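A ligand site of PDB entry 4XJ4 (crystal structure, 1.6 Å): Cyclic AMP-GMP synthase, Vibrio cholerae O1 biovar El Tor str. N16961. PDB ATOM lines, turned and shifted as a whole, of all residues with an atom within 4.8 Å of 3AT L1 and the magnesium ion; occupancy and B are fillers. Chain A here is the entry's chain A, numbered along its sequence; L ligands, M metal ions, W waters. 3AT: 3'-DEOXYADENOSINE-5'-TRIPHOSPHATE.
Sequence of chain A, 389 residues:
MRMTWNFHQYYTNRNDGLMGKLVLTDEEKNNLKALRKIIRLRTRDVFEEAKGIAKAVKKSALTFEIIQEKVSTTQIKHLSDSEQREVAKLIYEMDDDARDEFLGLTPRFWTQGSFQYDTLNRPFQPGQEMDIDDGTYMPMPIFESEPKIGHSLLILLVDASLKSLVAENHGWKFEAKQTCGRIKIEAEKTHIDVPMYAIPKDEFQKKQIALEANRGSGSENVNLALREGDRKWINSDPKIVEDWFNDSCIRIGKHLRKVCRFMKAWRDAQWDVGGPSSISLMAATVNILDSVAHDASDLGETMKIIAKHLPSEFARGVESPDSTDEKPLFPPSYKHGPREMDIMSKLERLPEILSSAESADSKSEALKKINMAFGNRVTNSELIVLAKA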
ATOM      1  N   GLN A 112      -0.652  -7.253  -2.785  1.00  0.00           N
ATOM      2  CA  GLN A 112      -0.499  -8.564  -3.400  1.00  0.00           C
ATOM      3  C   GLN A 112       0.483  -9.330  -2.560  1.00  0.00           C
ATOM      4  O   GLN A 112       1.006  -8.813  -1.579  1.00  0.00           O
ATOM      5  CB  GLN A 112      -0.002  -8.434  -4.856  1.00  0.00           C
ATOM      6  CG  GLN A 112       1.311  -7.700  -4.989  1.00  0.00           C
ATOM      7  CD  GLN A 112       1.738  -7.529  -6.452  1.00  0.00           C
ATOM      8  OE1 GLN A 112       2.719  -8.138  -6.900  1.00  0.00           O
ATOM      9  NE2 GLN A 112       0.988  -6.743  -7.211  1.00  0.00           N
ATOM     10  N   GLY A 113       0.742 -10.582  -2.925  1.00  0.00           N
ATOM     11  CA  GLY A 113       1.812 -11.306  -2.269  1.00  0.00           C
ATOM     12  C   GLY A 113       1.435 -11.823  -0.888  1.00  0.00           C
ATOM     13  O   GLY A 113       0.269 -11.875  -0.538  1.00  0.00           O
ATOM     14  N   SER A 114       2.448 -12.233  -0.125  1.00  0.00           N
ATOM     15  CA  SER A 114       2.207 -13.001   1.074  1.00  0.00           C
ATOM     16  C   SER A 114       1.518 -12.196   2.171  1.00  0.00           C
ATOM     17  O   SER A 114       0.916 -12.801   3.051  1.00  0.00           O
ATOM     18  CB  SER A 114       3.508 -13.629   1.594  1.00  0.00           C
ATOM     19  OG  SER A 114       4.480 -12.640   1.906  1.00  0.00           O
ATOM     20  N   TYR A 117      -2.330 -12.911   1.027  1.00  0.00           N
ATOM     21  CA  TYR A 117      -2.937 -14.202   1.290  1.00  0.00           C
ATOM     22  C   TYR A 117      -2.295 -14.947   2.480  1.00  0.00           C
ATOM     23  O   TYR A 117      -2.396 -16.167   2.591  1.00  0.00           O
ATOM     24  CB  TYR A 117      -2.913 -15.061   0.041  1.00  0.00           C
ATOM     25  CG  TYR A 117      -1.700 -14.869  -0.851  1.00  0.00           C
ATOM     26  CD1 TYR A 117      -0.480 -15.385  -0.472  1.00  0.00           C
ATOM     27  CD2 TYR A 117      -1.814 -14.271  -2.104  1.00  0.00           C
ATOM     28  CE1 TYR A 117       0.636 -15.255  -1.312  1.00  0.00           C
ATOM     29  CE2 TYR A 117      -0.711 -14.120  -2.944  1.00  0.00           C
ATOM     30  CZ  TYR A 117       0.511 -14.629  -2.529  1.00  0.00           C
ATOM     31  OH  TYR A 117       1.610 -14.533  -3.309  1.00  0.00           O
ATOM     32  N   THR A 119       0.800 -15.548   4.127  1.00  0.00           N
ATOM     33  CA  THR A 119       1.884 -16.538   4.177  1.00  0.00           C
ATOM     34  C   THR A 119       3.199 -15.823   4.437  1.00  0.00           C
ATOM     35  O   THR A 119       4.284 -16.354   4.119  1.00  0.00           O
ATOM     36  CB  THR A 119       1.990 -17.335   2.873  1.00  0.00           C
ATOM     37  OG1 THR A 119       2.103 -16.393   1.796  1.00  0.00           O
ATOM     38  CG2 THR A 119       0.765 -18.224   2.643  1.00  0.00           C
ATOM     39  N   LEU A 120       3.131 -14.633   5.029  1.00  0.00           N
ATOM     40  CA  LEU A 120       4.362 -13.842   5.246  1.00  0.00           C
ATOM     41  C   LEU A 120       5.095 -14.314   6.505  1.00  0.00           C
ATOM     42  O   LEU A 120       4.543 -14.256   7.620  1.00  0.00           O
ATOM     43  CB  LEU A 120       4.038 -12.348   5.345  1.00  0.00           C
ATOM     44  CG  LEU A 120       5.207 -11.425   5.669  1.00  0.00           C
ATOM     45  CD1 LEU A 120       6.336 -11.532   4.649  1.00  0.00           C
ATOM     46  CD2 LEU A 120       4.723  -9.968   5.769  1.00  0.00           C
ATOM     47  N   ASP A 131       8.715  -8.503   3.450  1.00  0.00           N
ATOM     48  CA  ASP A 131       8.160  -7.382   2.703  1.00  0.00           C
ATOM     49  C   ASP A 131       6.679  -7.436   2.500  1.00  0.00           C
ATOM     50  O   ASP A 131       6.011  -8.450   2.709  1.00  0.00           O
ATOM     51  CB  ASP A 131       8.853  -7.193   1.334  1.00  0.00           C
ATOM     52  CG  ASP A 131       8.700  -8.371   0.371  1.00  0.00           C
ATOM     53  OD1 ASP A 131       7.705  -9.104   0.397  1.00  0.00           O
ATOM     54  OD2 ASP A 131       9.580  -8.536  -0.485  1.00  0.00           O
ATOM     55  N   ASP A 133       4.013  -6.185  -0.431  1.00  0.00           N
ATOM     56  CA  ASP A 133       3.945  -5.817  -1.837  1.00  0.00           C
ATOM     57  C   ASP A 133       2.671  -5.048  -2.091  1.00  0.00           C
ATOM     58  O   ASP A 133       1.582  -5.635  -2.120  1.00  0.00           O
ATOM     59  CB  ASP A 133       4.005  -7.066  -2.714  1.00  0.00           C
ATOM     60  CG  ASP A 133       5.180  -7.937  -2.396  1.00  0.00           C
ATOM     61  OD1 ASP A 133       6.284  -7.531  -2.780  1.00  0.00           O
ATOM     62  OD2 ASP A 133       4.997  -9.033  -1.779  1.00  0.00           O
ATOM     63  N   SER A 236       0.072  -8.700 -16.785  1.00  0.00           N
ATOM     64  CA  SER A 236       0.231  -9.535 -15.600  1.00  0.00           C
ATOM     65  C   SER A 236      -0.699  -9.067 -14.494  1.00  0.00           C
ATOM     66  O   SER A 236      -0.378  -8.124 -13.786  1.00  0.00           O
ATOM     67  CB  SER A 236       1.680  -9.503 -15.102  1.00  0.00           C
ATOM     68  OG  SER A 236       1.881 -10.412 -14.016  1.00  0.00           O
ATOM     69  N   PRO A 238      -2.109  -9.431 -11.004  1.00  0.00           N
ATOM     70  CA  PRO A 238      -1.776 -10.134  -9.760  1.00  0.00           C
ATOM     71  C   PRO A 238      -2.986 -10.808  -9.125  1.00  0.00           C
ATOM     72  O   PRO A 238      -2.797 -11.714  -8.328  1.00  0.00           O
ATOM     73  CB  PRO A 238      -1.243  -9.019  -8.856  1.00  0.00           C
ATOM     74  CG  PRO A 238      -1.842  -7.763  -9.384  1.00  0.00           C
ATOM     75  CD  PRO A 238      -2.019  -7.959 -10.862  1.00  0.00           C
ATOM     76  N   VAL A 241      -3.229 -14.677  -9.485  1.00  0.00           N
ATOM     77  CA  VAL A 241      -2.510 -15.480  -8.482  1.00  0.00           C
ATOM     78  C   VAL A 241      -3.247 -15.484  -7.163  1.00  0.00           C
ATOM     79  O   VAL A 241      -3.380 -16.522  -6.527  1.00  0.00           O
ATOM     80  CB  VAL A 241      -1.071 -14.974  -8.281  1.00  0.00           C
ATOM     81  CG1 VAL A 241      -0.441 -15.642  -7.052  1.00  0.00           C
ATOM     82  CG2 VAL A 241      -0.240 -15.311  -9.501  1.00  0.00           C
ATOM     83  N   LYS A 264       8.744 -22.081   2.456  1.00  0.00           N
ATOM     84  CA  LYS A 264       9.473 -20.819   2.411  1.00  0.00           C
ATOM     85  C   LYS A 264      10.487 -20.706   3.556  1.00  0.00           C
ATOM     86  O   LYS A 264      11.580 -20.143   3.368  1.00  0.00           O
ATOM     87  CB  LYS A 264       8.493 -19.636   2.427  1.00  0.00           C
ATOM     88  CG  LYS A 264       7.691 -19.593   1.154  1.00  0.00           C
ATOM     89  CD  LYS A 264       6.440 -18.713   1.277  1.00  0.00           C
ATOM     90  CE  LYS A 264       6.812 -17.290   1.582  1.00  0.00           C
ATOM     91  NZ  LYS A 264       5.555 -16.429   1.696  1.00  0.00           N
ATOM     92  N   ARG A 267      13.447 -22.608   2.540  1.00  0.00           N
ATOM     93  CA  ARG A 267      14.216 -21.837   1.540  1.00  0.00           C
ATOM     94  C   ARG A 267      15.073 -20.764   2.242  1.00  0.00           C
ATOM     95  O   ARG A 267      16.265 -20.576   1.935  1.00  0.00           O
ATOM     96  CB  ARG A 267      13.217 -21.220   0.550  1.00  0.00           C
ATOM     97  CG  ARG A 267      13.830 -20.480  -0.648  1.00  0.00           C
ATOM     98  CD  ARG A 267      13.952 -18.995  -0.429  1.00  0.00           C
ATOM     99  NE  ARG A 267      12.865 -18.347   0.335  1.00  0.00           N
ATOM    100  CZ  ARG A 267      11.704 -17.904  -0.155  1.00  0.00           C
ATOM    101  NH1 ARG A 267      11.384 -18.042  -1.435  1.00  0.00           N
ATOM    102  NH2 ARG A 267      10.824 -17.347   0.686  1.00  0.00           N
ATOM    103  N   SER A 278       9.178 -17.674  -3.963  1.00  0.00           N
ATOM    104  CA  SER A 278       8.043 -18.082  -3.160  1.00  0.00           C
ATOM    105  C   SER A 278       6.889 -18.603  -4.041  1.00  0.00           C
ATOM    106  O   SER A 278       6.248 -19.599  -3.677  1.00  0.00           O
ATOM    107  CB  SER A 278       7.620 -16.883  -2.308  1.00  0.00           C
ATOM    108  OG  SER A 278       8.666 -16.686  -1.353  1.00  0.00           O
ATOM    109  N   ILE A 279       6.635 -17.961  -5.162  1.00  0.00           N
ATOM    110  CA  ILE A 279       5.499 -18.346  -5.995  1.00  0.00           C
ATOM    111  C   ILE A 279       5.786 -19.706  -6.650  1.00  0.00           C
ATOM    112  O   ILE A 279       4.880 -20.515  -6.845  1.00  0.00           O
ATOM    113  CB  ILE A 279       5.149 -17.275  -7.057  1.00  0.00           C
ATOM    114  CG1 ILE A 279       3.857 -17.623  -7.797  1.00  0.00           C
ATOM    115  CG2 ILE A 279       6.322 -17.064  -8.055  1.00  0.00           C
ATOM    116  CD1 ILE A 279       3.334 -16.491  -8.703  1.00  0.00           C
ATOM    117  N   MET A 282       4.931 -22.234  -4.011  1.00  0.00           N
ATOM    118  CA  MET A 282       3.468 -22.357  -3.836  1.00  0.00           C
ATOM    119  C   MET A 282       2.872 -23.192  -4.967  1.00  0.00           C
ATOM    120  O   MET A 282       2.017 -24.065  -4.720  1.00  0.00           O
ATOM    121  CB  MET A 282       2.820 -20.982  -3.797  1.00  0.00           C
ATOM    122  CG  MET A 282       3.244 -20.146  -2.628  1.00  0.00           C
ATOM    123  SD  MET A 282       2.827 -18.409  -2.935  1.00  0.00           S
ATOM    124  CE  MET A 282       1.057 -18.523  -3.182  1.00  0.00           C
ATOM    125  N   SER A 320       3.560 -21.216 -14.211  1.00  0.00           N
ATOM    126  CA  SER A 320       2.742 -20.226 -13.538  1.00  0.00           C
ATOM    127  C   SER A 320       1.264 -20.605 -13.548  1.00  0.00           C
ATOM    128  O   SER A 320       0.743 -21.141 -14.545  1.00  0.00           O
ATOM    129  CB  SER A 320       2.898 -18.846 -14.196  1.00  0.00           C
ATOM    130  OG  SER A 320       2.043 -17.915 -13.525  1.00  0.00           O
ATOM    131  N   ASP A 325       0.926 -16.654 -19.024  1.00  0.00           N
ATOM    132  CA  ASP A 325       2.367 -16.490 -18.819  1.00  0.00           C
ATOM    133  C   ASP A 325       3.078 -17.771 -19.193  1.00  0.00           C
ATOM    134  O   ASP A 325       2.995 -18.787 -18.468  1.00  0.00           O
ATOM    135  CB  ASP A 325       2.687 -16.135 -17.357  1.00  0.00           C
ATOM    136  CG  ASP A 325       4.144 -15.720 -17.154  1.00  0.00           C
ATOM    137  OD1 ASP A 325       4.952 -15.775 -18.120  1.00  0.00           O
ATOM    138  OD2 ASP A 325       4.487 -15.342 -16.017  1.00  0.00           O
ATOM    139  N   LEU A 329       7.990 -20.382 -13.742  1.00  0.00           N
ATOM    140  CA  LEU A 329       8.384 -19.847 -12.442  1.00  0.00           C
ATOM    141  C   LEU A 329       9.771 -20.378 -12.038  1.00  0.00           C
ATOM    142  O   LEU A 329      10.460 -19.781 -11.232  1.00  0.00           O
ATOM    143  CB  LEU A 329       7.333 -20.215 -11.387  1.00  0.00           C
ATOM    144  CG  LEU A 329       5.938 -19.664 -11.647  1.00  0.00           C
ATOM    145  CD1 LEU A 329       4.973 -20.146 -10.565  1.00  0.00           C
ATOM    146  CD2 LEU A 329       5.986 -18.125 -11.716  1.00  0.00           C
HETATM  147  PG  3AT L   1       7.449 -13.589   0.213  1.00  0.00           P
HETATM  148  O1G 3AT L   1       7.632 -12.089  -0.045  1.00  0.00           O
HETATM  149  O2G 3AT L   1       6.763 -13.883   1.518  1.00  0.00           O
HETATM  150  O3G 3AT L   1       8.736 -14.350  -0.025  1.00  0.00           O
HETATM  151  PB  3AT L   1       5.282 -13.518  -1.849  1.00  0.00           P
HETATM  152  O1B 3AT L   1       4.984 -12.073  -1.376  1.00  0.00           O
HETATM  153  O2B 3AT L   1       4.154 -14.460  -2.067  1.00  0.00           O
HETATM  154  O3B 3AT L   1       6.426 -14.187  -0.883  1.00  0.00           O
HETATM  155  PA  3AT L   1       6.866 -12.255  -3.882  1.00  0.00           P
HETATM  156  O1A 3AT L   1       7.298 -11.142  -2.930  1.00  0.00           O
HETATM  157  O2A 3AT L   1       7.973 -12.962  -4.655  1.00  0.00           O
HETATM  158  O3A 3AT L   1       6.070 -13.472  -3.213  1.00  0.00           O
HETATM  159  O5' 3AT L   1       5.746 -11.818  -4.962  1.00  0.00           O
HETATM  160  C5' 3AT L   1       4.589 -11.037  -4.630  1.00  0.00           C
HETATM  161  C4' 3AT L   1       3.492 -11.183  -5.705  1.00  0.00           C
HETATM  162  O4' 3AT L   1       3.984 -10.766  -6.982  1.00  0.00           O
HETATM  163  C3' 3AT L   1       2.969 -12.591  -5.910  1.00  0.00           C
HETATM  164  C2' 3AT L   1       2.561 -12.592  -7.375  1.00  0.00           C
HETATM  165  O2' 3AT L   1       1.240 -12.042  -7.516  1.00  0.00           O
HETATM  166  C1' 3AT L   1       3.512 -11.610  -8.029  1.00  0.00           C
HETATM  167  N9  3AT L   1       4.653 -12.329  -8.653  1.00  0.00           N
HETATM  168  C8  3AT L   1       5.929 -12.449  -8.230  1.00  0.00           C
HETATM  169  N7  3AT L   1       6.686 -13.181  -9.109  1.00  0.00           N
HETATM  170  C5  3AT L   1       5.867 -13.509 -10.117  1.00  0.00           C
HETATM  171  C6  3AT L   1       5.981 -14.269 -11.374  1.00  0.00           C
HETATM  172  N6  3AT L   1       7.170 -14.820 -11.720  1.00  0.00           N
HETATM  173  N1  3AT L   1       4.857 -14.359 -12.126  1.00  0.00           N
HETATM  174  C2  3AT L   1       3.692 -13.817 -11.798  1.00  0.00           C
HETATM  175  N3  3AT L   1       3.502 -13.106 -10.665  1.00  0.00           N
HETATM  176  C4  3AT L   1       4.543 -12.941  -9.820  1.00  0.00           C
HETATM  177  PG  3AT L   2      15.541  -9.767  -6.991  1.00  0.00           P
HETATM  178  O1G 3AT L   2      15.469  -8.615  -6.015  1.00  0.00           O
HETATM  179  O2G 3AT L   2      16.882 -10.476  -7.016  1.00  0.00           O
HETATM  180  O3G 3AT L   2      14.992  -9.451  -8.362  1.00  0.00           O
HETATM  181  PB  3AT L   2      13.303 -10.532  -5.392  1.00  0.00           P
HETATM  182  O1B 3AT L   2      13.823  -9.750  -4.198  1.00  0.00           O
HETATM  183  O2B 3AT L   2      12.555 -11.819  -5.137  1.00  0.00           O
HETATM  184  O3B 3AT L   2      14.535 -10.875  -6.384  1.00  0.00           O
HETATM  185  PA  3AT L   2      11.847 -10.000  -7.781  1.00  0.00           P
HETATM  186  O1A 3AT L   2      12.322  -8.943  -8.764  1.00  0.00           O
HETATM  187  O2A 3AT L   2      12.202 -11.444  -8.023  1.00  0.00           O
HETATM  188  O3A 3AT L   2      12.391  -9.561  -6.314  1.00  0.00           O
HETATM  189  O5' 3AT L   2      10.239  -9.850  -7.724  1.00  0.00           O
HETATM  190  C5' 3AT L   2       9.500  -9.775  -6.508  1.00  0.00           C
HETATM  191  C4' 3AT L   2       8.436  -8.694  -6.714  1.00  0.00           C
HETATM  192  O4' 3AT L   2       8.052  -8.642  -8.092  1.00  0.00           O
HETATM  193  C3' 3AT L   2       7.166  -8.938  -5.921  1.00  0.00           C
HETATM  194  C2' 3AT L   2       6.058  -8.404  -6.827  1.00  0.00           C
HETATM  195  O2' 3AT L   2       5.607  -7.175  -6.250  1.00  0.00           O
HETATM  196  C1' 3AT L   2       6.701  -8.175  -8.194  1.00  0.00           C
HETATM  197  N9  3AT L   2       5.978  -8.773  -9.371  1.00  0.00           N
HETATM  198  C8  3AT L   2       4.654  -8.625  -9.621  1.00  0.00           C
HETATM  199  N7  3AT L   2       4.275  -9.253 -10.767  1.00  0.00           N
HETATM  200  C5  3AT L   2       5.379  -9.808 -11.299  1.00  0.00           C
HETATM  201  C6  3AT L   2       5.664 -10.606 -12.510  1.00  0.00           C
HETATM  202  N6  3AT L   2       4.677 -10.941 -13.373  1.00  0.00           N
HETATM  203  N1  3AT L   2       6.944 -11.008 -12.724  1.00  0.00           N
HETATM  204  C2  3AT L   2       7.930 -10.683 -11.862  1.00  0.00           C
HETATM  205  N3  3AT L   2       7.721  -9.961 -10.738  1.00  0.00           N
HETATM  206  C4  3AT L   2       6.494  -9.489 -10.396  1.00  0.00           C
HETATM  207 MG    MG M   1       6.365 -10.535  -0.866  1.00  0.00          MG
HETATM  208  O   HOH W   1       3.969 -16.698  -0.535  1.00  0.00           O
HETATM  209  O   HOH W   2       8.992 -11.412   2.710  1.00  0.00           O
HETATM  210  O   HOH W   3      10.927 -13.912  -1.534  1.00  0.00           O
HETATM  211  O   HOH W   4      -1.046 -11.502  -5.515  1.00  0.00           O
HETATM  212  O   HOH W   5       8.832 -14.191  -8.160  1.00  0.00           O
HETATM  213  O   HOH W   6       9.928 -11.257  -0.812  1.00  0.00           O
HETATM  214  O   HOH W   7       2.778 -15.497 -14.139  1.00  0.00           O
HETATM  215  O   HOH W   8       7.858 -14.889   3.780  1.00  0.00           O
HETATM  216  O   HOH W   9       6.605 -16.164 -14.893  1.00  0.00           O
HETATM  217  O   HOH W  10       5.242 -10.269   0.834  1.00  0.00           O
HETATM  218  O   HOH W  11       7.660 -15.192  -5.597  1.00  0.00           O
HETATM  219  O   HOH W  12      11.082 -13.789   1.715  1.00  0.00           O
HETATM  220  O   HOH W  13      10.346 -15.097  -3.886  1.00  0.00           O
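The magnesium ion is bound by water W10.
The magnesium ion is bound by O1B of 3AT L1 (2.1 Å).
An oxygen (O1G) of 3AT L1 binds the magnesium ion.
The magnesium ion is bound by the side-chain carboxylate (OD2) of Asp 133 (2.2 Å).
OD1 of Asp 131 is bound to the magnesium ion (2.3 Å).
The magnesium ion is bound by O1A of 3AT L1, 2.3 Å away.
Residues that only touch the magnesium ion: Ser 114 (3.96 Å).
Along chain A the residues within 4 Å of the magnesium ion span positions 114 to 133.
The nearest printed residue that does not touch the magnesium ion is Gly 113 (4.8 Å).
Water W11 lies within hydrogen-bond range of an oxygen (O2A) of 3AT L1 (2.4 Å), the backbone NH (N) of Ile 279 (3.0 Å) and the backbone NH (N) of Ser 278 (3.3 Å).
Water W8 lies within hydrogen-bond range of an oxygen (O2G) of 3AT L1 (2.7 Å) and the side-chain amino group of Lys 264 (3.5 Å).
Water W1 lies within hydrogen-bond range of an oxygen (O2B) of 3AT L1 (2.7 Å), the side-chain amino group of Lys 264 (2.8 Å), the side-chain hydroxyl of Thr 119 (3.0 Å) and the side-chain sulfur of Met 282 (3.2 Å).
Water W7 lies within hydrogen-bond range of OD2 of Asp 325, OG of Ser 320 and N1 of 3AT L1.
Water W4 lies within hydrogen-bond range of an oxygen (O2') of 3AT L1, the backbone NH (N) of Gly 113 and the backbone carbonyl oxygen (O) of Pro 238.
Water W13 bridges the backbone NH of Ser 278 and an oxygen (O2A) of 3AT L1.
O of Asp 133 sits at hydrogen-bond distance from N of Gln 112 (2.8 Å).
The backbone carbonyl oxygen of Ser 114 lies within hydrogen-bond range of the backbone NH of Leu 120, at 3.5 Å.
O of Ser 114 is in hydrogen-bond range of N of Thr 119 (3.0 Å).
NH1 of Arg 267 sits at hydrogen-bond distance from OG of Ser 278, 3.0 Å away.
The side-chain amino group (NZ) of Lys 264 lies within hydrogen-bond range of the backbone carbonyl oxygen (O) of Thr 119.
An oxygen (O2B) of 3AT L1 sits at hydrogen-bond distance from the backbone NH (N) of Ser 114 (3.4 Å).
The side-chain hydroxyl (OG) of Ser 114 lies within hydrogen-bond range of an oxygen (O2G) of 3AT L1 (2.6 Å).
OG of Ser 278 lies within hydrogen-bond range of O3G of 3AT L1, 2.7 Å away.
The side-chain amino group (NZ) of Lys 264 is in salt-bridge range of an oxygen (O2G) of 3AT L1 (2.8 Å).
The side-chain hydroxyl of Tyr 117 is in hydrogen-bond range of an oxygen (O2B) of 3AT L1, 2.8 Å away.
The side-chain amide oxygen (OE1) of Gln 112 sits close to an oxygen (O4') of 3AT L1, at 2.9 Å.
The guanidinium group of Arg 267 is in salt-bridge range of an oxygen (O3G) of 3AT L1, 3.7 Å away.
OE1 of Gln 112 is in hydrogen-bond range of O2' of 3AT L2 (3.1 Å).
N6 of 3AT L2 lies within hydrogen-bond range of OG of Ser 236 (2.9 Å).
Residues that only touch 3AT L1: Gly 113, Leu 329, Val 241, Ile 279 and Leu 120.
Hydrophobic or aromatic side chains within 4 Å of 3AT L1: Tyr 117, Leu 120, Val 241, Ile 279 and Leu 329.
13 residues have an atom within 4 Å of 3AT L1: Gln 112, Gly 113, Ser 114, Tyr 117, Leu 120, Asp 131, Asp 133, Val 241, Lys 264, Arg 267, Ser 278, Ile 279 and Leu 329.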
